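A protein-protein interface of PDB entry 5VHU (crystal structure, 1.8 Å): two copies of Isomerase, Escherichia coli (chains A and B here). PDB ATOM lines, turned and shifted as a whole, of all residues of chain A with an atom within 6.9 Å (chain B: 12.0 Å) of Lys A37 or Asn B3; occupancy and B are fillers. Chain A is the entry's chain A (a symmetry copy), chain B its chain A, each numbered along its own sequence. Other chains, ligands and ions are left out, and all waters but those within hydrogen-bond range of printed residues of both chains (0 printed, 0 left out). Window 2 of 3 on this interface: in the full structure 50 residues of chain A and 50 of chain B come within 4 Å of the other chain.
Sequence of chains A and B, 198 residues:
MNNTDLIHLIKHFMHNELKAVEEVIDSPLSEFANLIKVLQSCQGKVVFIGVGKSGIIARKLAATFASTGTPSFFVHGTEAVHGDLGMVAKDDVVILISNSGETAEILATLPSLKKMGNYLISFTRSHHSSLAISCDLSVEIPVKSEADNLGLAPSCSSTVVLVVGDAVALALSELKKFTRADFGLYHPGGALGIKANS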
ATOM      1  N   SER A  30     -27.794  22.738 -23.091  1.00  0.00           N
ATOM      2  CA  SER A  30     -28.321  24.051 -22.580  1.00  0.00           C
ATOM      3  C   SER A  30     -28.970  23.986 -21.201  1.00  0.00           C
ATOM      4  O   SER A  30     -28.780  24.886 -20.389  1.00  0.00           O
ATOM      5  CB  SER A  30     -29.360  24.647 -23.533  1.00  0.00           C
ATOM      6  OG  SER A  30     -28.734  24.823 -24.760  1.00  0.00           O
ATOM      7  N   PHE A  32     -28.379  22.084 -18.727  1.00  0.00           N
ATOM      8  CA  PHE A  32     -27.522  21.618 -17.624  1.00  0.00           C
ATOM      9  C   PHE A  32     -27.192  22.597 -16.542  1.00  0.00           C
ATOM     10  O   PHE A  32     -26.910  22.202 -15.395  1.00  0.00           O
ATOM     11  CB  PHE A  32     -26.279  20.944 -18.155  1.00  0.00           C
ATOM     12  CG  PHE A  32     -26.541  19.546 -18.597  1.00  0.00           C
ATOM     13  CD1 PHE A  32     -27.300  19.282 -19.725  1.00  0.00           C
ATOM     14  CD2 PHE A  32     -26.032  18.485 -17.872  1.00  0.00           C
ATOM     15  CE1 PHE A  32     -27.503  17.991 -20.183  1.00  0.00           C
ATOM     16  CE2 PHE A  32     -26.299  17.176 -18.275  1.00  0.00           C
ATOM     17  CZ  PHE A  32     -27.011  16.928 -19.442  1.00  0.00           C
ATOM     18  N   ALA A  33     -27.152  23.880 -16.914  1.00  0.00           N
ATOM     19  CA  ALA A  33     -26.882  24.903 -15.946  1.00  0.00           C
ATOM     20  C   ALA A  33     -28.062  24.961 -14.968  1.00  0.00           C
ATOM     21  O   ALA A  33     -27.867  25.047 -13.734  1.00  0.00           O
ATOM     22  CB  ALA A  33     -26.661  26.243 -16.657  1.00  0.00           C
ATOM     23  N   ASN A  34     -29.290  24.928 -15.523  1.00  0.00           N
ATOM     24  CA  ASN A  34     -30.519  24.874 -14.694  1.00  0.00           C
ATOM     25  C   ASN A  34     -30.539  23.614 -13.857  1.00  0.00           C
ATOM     26  O   ASN A  34     -30.937  23.655 -12.685  1.00  0.00           O
ATOM     27  CB  ASN A  34     -31.767  24.902 -15.549  1.00  0.00           C
ATOM     28  CG  ASN A  34     -32.106  26.313 -15.982  1.00  0.00           C
ATOM     29  OD1 ASN A  34     -31.567  27.267 -15.425  1.00  0.00           O
ATOM     30  ND2 ASN A  34     -32.976  26.454 -16.967  1.00  0.00           N
ATOM     31  N   LEU A  35     -30.115  22.503 -14.468  1.00  0.00           N
ATOM     32  CA  LEU A  35     -30.079  21.248 -13.712  1.00  0.00           C
ATOM     33  C   LEU A  35     -29.197  21.380 -12.445  1.00  0.00           C
ATOM     34  O   LEU A  35     -29.583  20.938 -11.357  1.00  0.00           O
ATOM     35  CB  LEU A  35     -29.611  20.089 -14.611  1.00  0.00           C
ATOM     36  CG  LEU A  35     -29.333  18.716 -13.929  1.00  0.00           C
ATOM     37  CD1 LEU A  35     -30.652  18.066 -13.374  1.00  0.00           C
ATOM     38  CD2 LEU A  35     -28.659  17.792 -14.929  1.00  0.00           C
ATOM     39  N   ILE A  36     -28.005  21.946 -12.603  1.00  0.00           N
ATOM     40  CA  ILE A  36     -27.065  22.121 -11.470  1.00  0.00           C
ATOM     41  C   ILE A  36     -27.720  22.982 -10.391  1.00  0.00           C
ATOM     42  O   ILE A  36     -27.668  22.671  -9.205  1.00  0.00           O
ATOM     43  CB  ILE A  36     -25.696  22.693 -11.934  1.00  0.00           C
ATOM     44  CG1 ILE A  36     -24.914  21.637 -12.760  1.00  0.00           C
ATOM     45  CG2 ILE A  36     -24.858  23.215 -10.741  1.00  0.00           C
ATOM     46  CD1 ILE A  36     -24.350  20.471 -11.932  1.00  0.00           C
ATOM     47  N   LYS A  37     -28.356  24.073 -10.816  1.00  0.00           N
ATOM     48  CA  LYS A  37     -28.986  24.968  -9.858  1.00  0.00           C
ATOM     49  C   LYS A  37     -30.061  24.331  -9.021  1.00  0.00           C
ATOM     50  O   LYS A  37     -30.121  24.565  -7.777  1.00  0.00           O
ATOM     51  CB  LYS A  37     -29.498  26.227 -10.576  1.00  0.00           C
ATOM     52  CG  LYS A  37     -28.273  27.057 -10.977  1.00  0.00           C
ATOM     53  CD  LYS A  37     -28.604  28.134 -12.010  1.00  0.00           C
ATOM     54  CE  LYS A  37     -27.314  28.884 -12.347  1.00  0.00           C
ATOM     55  NZ  LYS A  37     -27.634  29.892 -13.389  1.00  0.00           N
ATOM     56  N   VAL A  38     -30.934  23.555  -9.683  1.00  0.00           N
ATOM     57  CA  VAL A  38     -32.007  22.844  -8.985  1.00  0.00           C
ATOM     58  C   VAL A  38     -31.396  21.878  -7.977  1.00  0.00           C
ATOM     59  O   VAL A  38     -31.882  21.749  -6.854  1.00  0.00           O
ATOM     60  CB  VAL A  38     -32.939  22.062  -9.950  1.00  0.00           C
ATOM     61  CG1 VAL A  38     -33.926  21.140  -9.185  1.00  0.00           C
ATOM     62  CG2 VAL A  38     -33.697  23.039 -10.872  1.00  0.00           C
ATOM     63  N   LEU A  39     -30.349  21.161  -8.399  1.00  0.00           N
ATOM     64  CA  LEU A  39     -29.728  20.112  -7.522  1.00  0.00           C
ATOM     65  C   LEU A  39     -28.997  20.751  -6.348  1.00  0.00           C
ATOM     66  O   LEU A  39     -29.069  20.250  -5.223  1.00  0.00           O
ATOM     67  CB  LEU A  39     -28.836  19.184  -8.346  1.00  0.00           C
ATOM     68  CG  LEU A  39     -29.614  18.321  -9.338  1.00  0.00           C
ATOM     69  CD1 LEU A  39     -28.614  17.462 -10.154  1.00  0.00           C
ATOM     70  CD2 LEU A  39     -30.616  17.357  -8.641  1.00  0.00           C
ATOM     71  N   GLN A  40     -28.380  21.906  -6.575  1.00  0.00           N
ATOM     72  CA  GLN A  40     -27.759  22.661  -5.464  1.00  0.00           C
ATOM     73  C   GLN A  40     -28.780  23.190  -4.447  1.00  0.00           C
ATOM     74  O   GLN A  40     -28.454  23.359  -3.274  1.00  0.00           O
ATOM     75  CB  GLN A  40     -27.008  23.874  -6.024  1.00  0.00           C
ATOM     76  CG  GLN A  40     -25.698  23.475  -6.672  1.00  0.00           C
ATOM     77  CD  GLN A  40     -24.941  24.679  -7.249  1.00  0.00           C
ATOM     78  OE1 GLN A  40     -25.507  25.558  -7.884  1.00  0.00           O
ATOM     79  NE2 GLN A  40     -23.653  24.703  -7.008  1.00  0.00           N
ATOM     80  N   SER A  41     -29.987  23.491  -4.902  1.00  0.00           N
ATOM     81  CA  SER A  41     -31.048  24.007  -4.065  1.00  0.00           C
ATOM     82  C   SER A  41     -31.701  22.895  -3.203  1.00  0.00           C
ATOM     83  O   SER A  41     -32.421  23.197  -2.245  1.00  0.00           O
ATOM     84  CB  SER A  41     -32.100  24.701  -4.955  1.00  0.00           C
ATOM     85  OG  SER A  41     -33.094  23.740  -5.368  1.00  0.00           O
ATOM     86  N   CYS A  42     -31.496  21.617  -3.553  1.00  0.00           N
ATOM     87  CA  CYS A  42     -32.113  20.503  -2.820  1.00  0.00           C
ATOM     88  C   CYS A  42     -31.722  20.473  -1.340  1.00  0.00           C
ATOM     89  O   CYS A  42     -30.554  20.352  -1.018  1.00  0.00           O
ATOM     90  CB  CYS A  42     -31.804  19.179  -3.515  1.00  0.00           C
ATOM     91  SG  CYS A  42     -32.611  17.722  -2.793  1.00  0.00           S
ATOM     92  N   LEU A 172     -21.192  19.015  -9.064  1.00  0.00           N
ATOM     93  CA  LEU A 172     -21.839  19.422  -7.793  1.00  0.00           C
ATOM     94  C   LEU A 172     -20.804  19.318  -6.674  1.00  0.00           C
ATOM     95  O   LEU A 172     -20.710  20.236  -5.807  1.00  0.00           O
ATOM     96  CB  LEU A 172     -23.055  18.527  -7.469  1.00  0.00           C
ATOM     97  CG  LEU A 172     -24.255  18.780  -8.390  1.00  0.00           C
ATOM     98  CD1 LEU A 172     -25.252  17.634  -8.108  1.00  0.00           C
ATOM     99  CD2 LEU A 172     -24.880  20.134  -8.017  1.00  0.00           C
ATOM    100  N   MET B   1     -20.427  30.477 -10.451  1.00  0.00           N
ATOM    101  CA  MET B   1     -19.908  30.120 -11.777  1.00  0.00           C
ATOM    102  C   MET B   1     -21.022  30.407 -12.777  1.00  0.00           C
ATOM    103  O   MET B   1     -22.159  29.967 -12.553  1.00  0.00           O
ATOM    104  CB  MET B   1     -19.524  28.634 -11.749  1.00  0.00           C
ATOM    105  CG  MET B   1     -18.761  28.200 -12.958  1.00  0.00           C
ATOM    106  SD  MET B   1     -18.110  26.537 -12.828  1.00  0.00           S
ATOM    107  CE  MET B   1     -16.648  26.757 -11.805  1.00  0.00           C
ATOM    108  N   ASN B   2     -20.745  31.173 -13.853  1.00  0.00           N
ATOM    109  CA  ASN B   2     -21.773  31.423 -14.916  1.00  0.00           C
ATOM    110  C   ASN B   2     -22.141  30.138 -15.697  1.00  0.00           C
ATOM    111  O   ASN B   2     -21.472  29.119 -15.558  1.00  0.00           O
ATOM    112  CB  ASN B   2     -21.378  32.566 -15.889  1.00  0.00           C
ATOM    113  CG  ASN B   2     -20.174  32.226 -16.788  1.00  0.00           C
ATOM    114  OD1 ASN B   2     -19.746  31.086 -16.922  1.00  0.00           O
ATOM    115  ND2 ASN B   2     -19.636  33.242 -17.433  1.00  0.00           N
ATOM    116  N   ASN B   3     -23.171  30.215 -16.527  1.00  0.00           N
ATOM    117  CA  ASN B   3     -23.703  29.062 -17.264  1.00  0.00           C
ATOM    118  C   ASN B   3     -22.720  28.441 -18.232  1.00  0.00           C
ATOM    119  O   ASN B   3     -22.584  27.189 -18.270  1.00  0.00           O
ATOM    120  CB  ASN B   3     -25.012  29.425 -17.957  1.00  0.00           C
ATOM    121  CG  ASN B   3     -26.136  29.736 -16.960  1.00  0.00           C
ATOM    122  OD1 ASN B   3     -25.974  29.617 -15.731  1.00  0.00           O
ATOM    123  ND2 ASN B   3     -27.283  30.137 -17.488  1.00  0.00           N
ATOM    124  N   THR B   4     -21.987  29.270 -18.987  1.00  0.00           N
ATOM    125  CA  THR B   4     -21.042  28.704 -19.947  1.00  0.00           C
ATOM    126  C   THR B   4     -19.874  27.976 -19.212  1.00  0.00           C
ATOM    127  O   THR B   4     -19.432  26.897 -19.646  1.00  0.00           O
ATOM    128  CB  THR B   4     -20.607  29.692 -21.085  1.00  0.00           C
ATOM    129  OG1 THR B   4     -19.837  30.745 -20.544  1.00  0.00           O
ATOM    130  CG2 THR B   4     -21.823  30.291 -21.839  1.00  0.00           C
ATOM    131  N   ASP B   5     -19.455  28.501 -18.061  1.00  0.00           N
ATOM    132  CA  ASP B   5     -18.393  27.861 -17.288  1.00  0.00           C
ATOM    133  C   ASP B   5     -18.867  26.541 -16.616  1.00  0.00           C
ATOM    134  O   ASP B   5     -18.065  25.590 -16.564  1.00  0.00           O
ATOM    135  CB  ASP B   5     -17.828  28.789 -16.212  1.00  0.00           C
ATOM    136  CG  ASP B   5     -16.919  29.869 -16.770  1.00  0.00           C
ATOM    137  OD1 ASP B   5     -16.569  29.840 -17.957  1.00  0.00           O
ATOM    138  OD2 ASP B   5     -16.566  30.763 -15.991  1.00  0.00           O
ATOM    139  N   LEU B   6     -20.120  26.508 -16.100  1.00  0.00           N
ATOM    140  CA  LEU B   6     -20.747  25.264 -15.546  1.00  0.00           C
ATOM    141  C   LEU B   6     -20.779  24.198 -16.627  1.00  0.00           C
ATOM    142  O   LEU B   6     -20.405  23.026 -16.364  1.00  0.00           O
ATOM    143  CB  LEU B   6     -22.199  25.434 -15.047  1.00  0.00           C
ATOM    144  CG  LEU B   6     -22.650  26.108 -13.730  1.00  0.00           C
ATOM    145  CD1 LEU B   6     -24.186  26.193 -13.660  1.00  0.00           C
ATOM    146  CD2 LEU B   6     -22.097  25.429 -12.467  1.00  0.00           C
ATOM    147  N   ILE B   7     -21.238  24.584 -17.831  1.00  0.00           N
ATOM    148  CA  ILE B   7     -21.276  23.614 -18.980  1.00  0.00           C
ATOM    149  C   ILE B   7     -19.892  23.058 -19.309  1.00  0.00           C
ATOM    150  O   ILE B   7     -19.736  21.822 -19.531  1.00  0.00           O
ATOM    151  CB  ILE B   7     -22.092  24.159 -20.205  1.00  0.00           C
ATOM    152  CG1 ILE B   7     -23.587  24.261 -19.817  1.00  0.00           C
ATOM    153  CG2 ILE B   7     -21.895  23.301 -21.462  1.00  0.00           C
ATOM    154  CD1 ILE B   7     -24.471  25.008 -20.826  1.00  0.00           C
ATOM    155  N   HIS B   8     -18.879  23.924 -19.305  1.00  0.00           N
ATOM    156  CA  HIS B   8     -17.504  23.508 -19.616  1.00  0.00           C
ATOM    157  C   HIS B   8     -16.978  22.598 -18.500  1.00  0.00           C
ATOM    158  O   HIS B   8     -16.205  21.673 -18.763  1.00  0.00           O
ATOM    159  CB  HIS B   8     -16.525  24.679 -19.907  1.00  0.00           C
ATOM    160  CG  HIS B   8     -16.676  25.301 -21.293  1.00  0.00           C
ATOM    161  ND1 HIS B   8     -16.882  24.561 -22.453  1.00  0.00           N
ATOM    162  CD2 HIS B   8     -16.615  26.600 -21.698  1.00  0.00           C
ATOM    163  CE1 HIS B   8     -16.977  25.377 -23.495  1.00  0.00           C
ATOM    164  NE2 HIS B   8     -16.824  26.620 -23.063  1.00  0.00           N
ATOM    165  N   LEU B   9     -17.448  22.812 -17.278  1.00  0.00           N
ATOM    166  CA  LEU B   9     -16.981  21.977 -16.160  1.00  0.00           C
ATOM    167  C   LEU B   9     -17.562  20.553 -16.329  1.00  0.00           C
ATOM    168  O   LEU B   9     -16.844  19.544 -16.263  1.00  0.00           O
ATOM    169  CB  LEU B   9     -17.384  22.617 -14.828  1.00  0.00           C
ATOM    170  CG  LEU B   9     -17.105  21.850 -13.542  1.00  0.00           C
ATOM    171  CD1 LEU B   9     -15.620  21.618 -13.319  1.00  0.00           C
ATOM    172  CD2 LEU B   9     -17.736  22.559 -12.363  1.00  0.00           C
ATOM    173  N   ILE B  10     -18.866  20.482 -16.608  1.00  0.00           N
ATOM    174  CA  ILE B  10     -19.509  19.186 -16.908  1.00  0.00           C
ATOM    175  C   ILE B  10     -18.821  18.463 -18.082  1.00  0.00           C
ATOM    176  O   ILE B  10     -18.485  17.301 -17.974  1.00  0.00           O
ATOM    177  CB  ILE B  10     -21.031  19.385 -17.128  1.00  0.00           C
ATOM    178  CG1 ILE B  10     -21.675  19.830 -15.802  1.00  0.00           C
ATOM    179  CG2 ILE B  10     -21.682  18.156 -17.753  1.00  0.00           C
ATOM    180  CD1 ILE B  10     -23.040  20.514 -15.973  1.00  0.00           C
ATOM    181  N   LYS B  11     -18.585  19.154 -19.194  1.00  0.00           N
ATOM    182  CA  LYS B  11     -17.929  18.531 -20.337  1.00  0.00           C
ATOM    183  C   LYS B  11     -16.490  18.051 -20.019  1.00  0.00           C
ATOM    184  O   LYS B  11     -16.018  17.047 -20.563  1.00  0.00           O
ATOM    185  CB  LYS B  11     -17.924  19.523 -21.513  1.00  0.00           C
ATOM    186  CG  LYS B  11     -19.306  19.654 -22.129  1.00  0.00           C
ATOM    187  CD  LYS B  11     -19.263  20.549 -23.369  1.00  0.00           C
ATOM    188  CE  LYS B  11     -20.660  20.703 -23.966  1.00  0.00           C
ATOM    189  NZ  LYS B  11     -20.498  21.124 -25.399  1.00  0.00           N
ATOM    190  N   HIS B  12     -15.802  18.764 -19.141  1.00  0.00           N
ATOM    191  CA  HIS B  12     -14.455  18.347 -18.712  1.00  0.00           C
ATOM    192  C   HIS B  12     -14.481  16.939 -18.061  1.00  0.00           C
ATOM    193  O   HIS B  12     -13.625  16.082 -18.361  1.00  0.00           O
ATOM    194  CB  HIS B  12     -13.865  19.380 -17.738  1.00  0.00           C
ATOM    195  CG  HIS B  12     -12.701  18.888 -16.921  1.00  0.00           C
ATOM    196  ND1 HIS B  12     -11.421  18.778 -17.430  1.00  0.00           N
ATOM    197  CD2 HIS B  12     -12.627  18.480 -15.625  1.00  0.00           C
ATOM    198  CE1 HIS B  12     -10.606  18.331 -16.487  1.00  0.00           C
ATOM    199  NE2 HIS B  12     -11.310  18.145 -15.379  1.00  0.00           N
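The side-chain amide oxygen of Asn B3 lies within hydrogen-bond range of the side-chain amino group of Lys A37, at 2.9 Å.
Among the printed residues, merely in contact across the chains: Ala A33 with Asn B3, Ala A33 with Leu B6, Ile A36 with Ile B10, Phe A32 with Ile B10 and Ile A36 with Leu B6.
Of the 13 printed residues of chain A, 4 touch a printed residue of chain B. Of the 12 printed residues of chain B, 3 touch a printed residue of chain A. Hydrophobic or aromatic side chains of chain B within 4 Å of the printed part of chain A: Leu B6 and Ile B10. Among the printed residues, 6 pairs touch across the chains. Among the printed residues, no Asp or Glu carboxylate lies within 4 Å of a Lys or Arg side-chain nitrogen of the other chain.
Lys A37 touches just one residue of chain B: Asn B3. Printed residues of chain A within 4 Å of Asn B3: Ala A33 (3.5 Å) and Lys A37 (2.9 Å). No residue of chain B comes within 4 Å of Asn A34. Ile A36 touches just these residues of chain B: Leu B6 (3.9 Å) and Ile B10 (3.9 Å). No residue of chain B comes within 4 Å of Val A38. No residue of chain B comes within 4 Å of Leu A39. Gln A40 touches none of the printed residues of chain B. No residue of chain B comes within 4 Å of Ser A41. Printed residues of chain A within 4 Å of Leu B6: Ala A33 and Ile A36. Printed residues of chain B within 4 Å of Phe A32: Ile B10 (3.9 Å). Of the printed residues of chain A, Ile B10 touches Phe A32 (3.9 Å) and Ile A36 (3.9 Å). The nearest residue of chain B that does not touch Lys A37 is Leu B6 (4.3 Å). The nearest residue of chain A that does not touch Asn B3 is Asn A34 (5.6 Å).
No position is printed for both chains. Of the 6 pairs that touch across the chains among the printed residues, none has its exchanged pair printed and touching as well.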
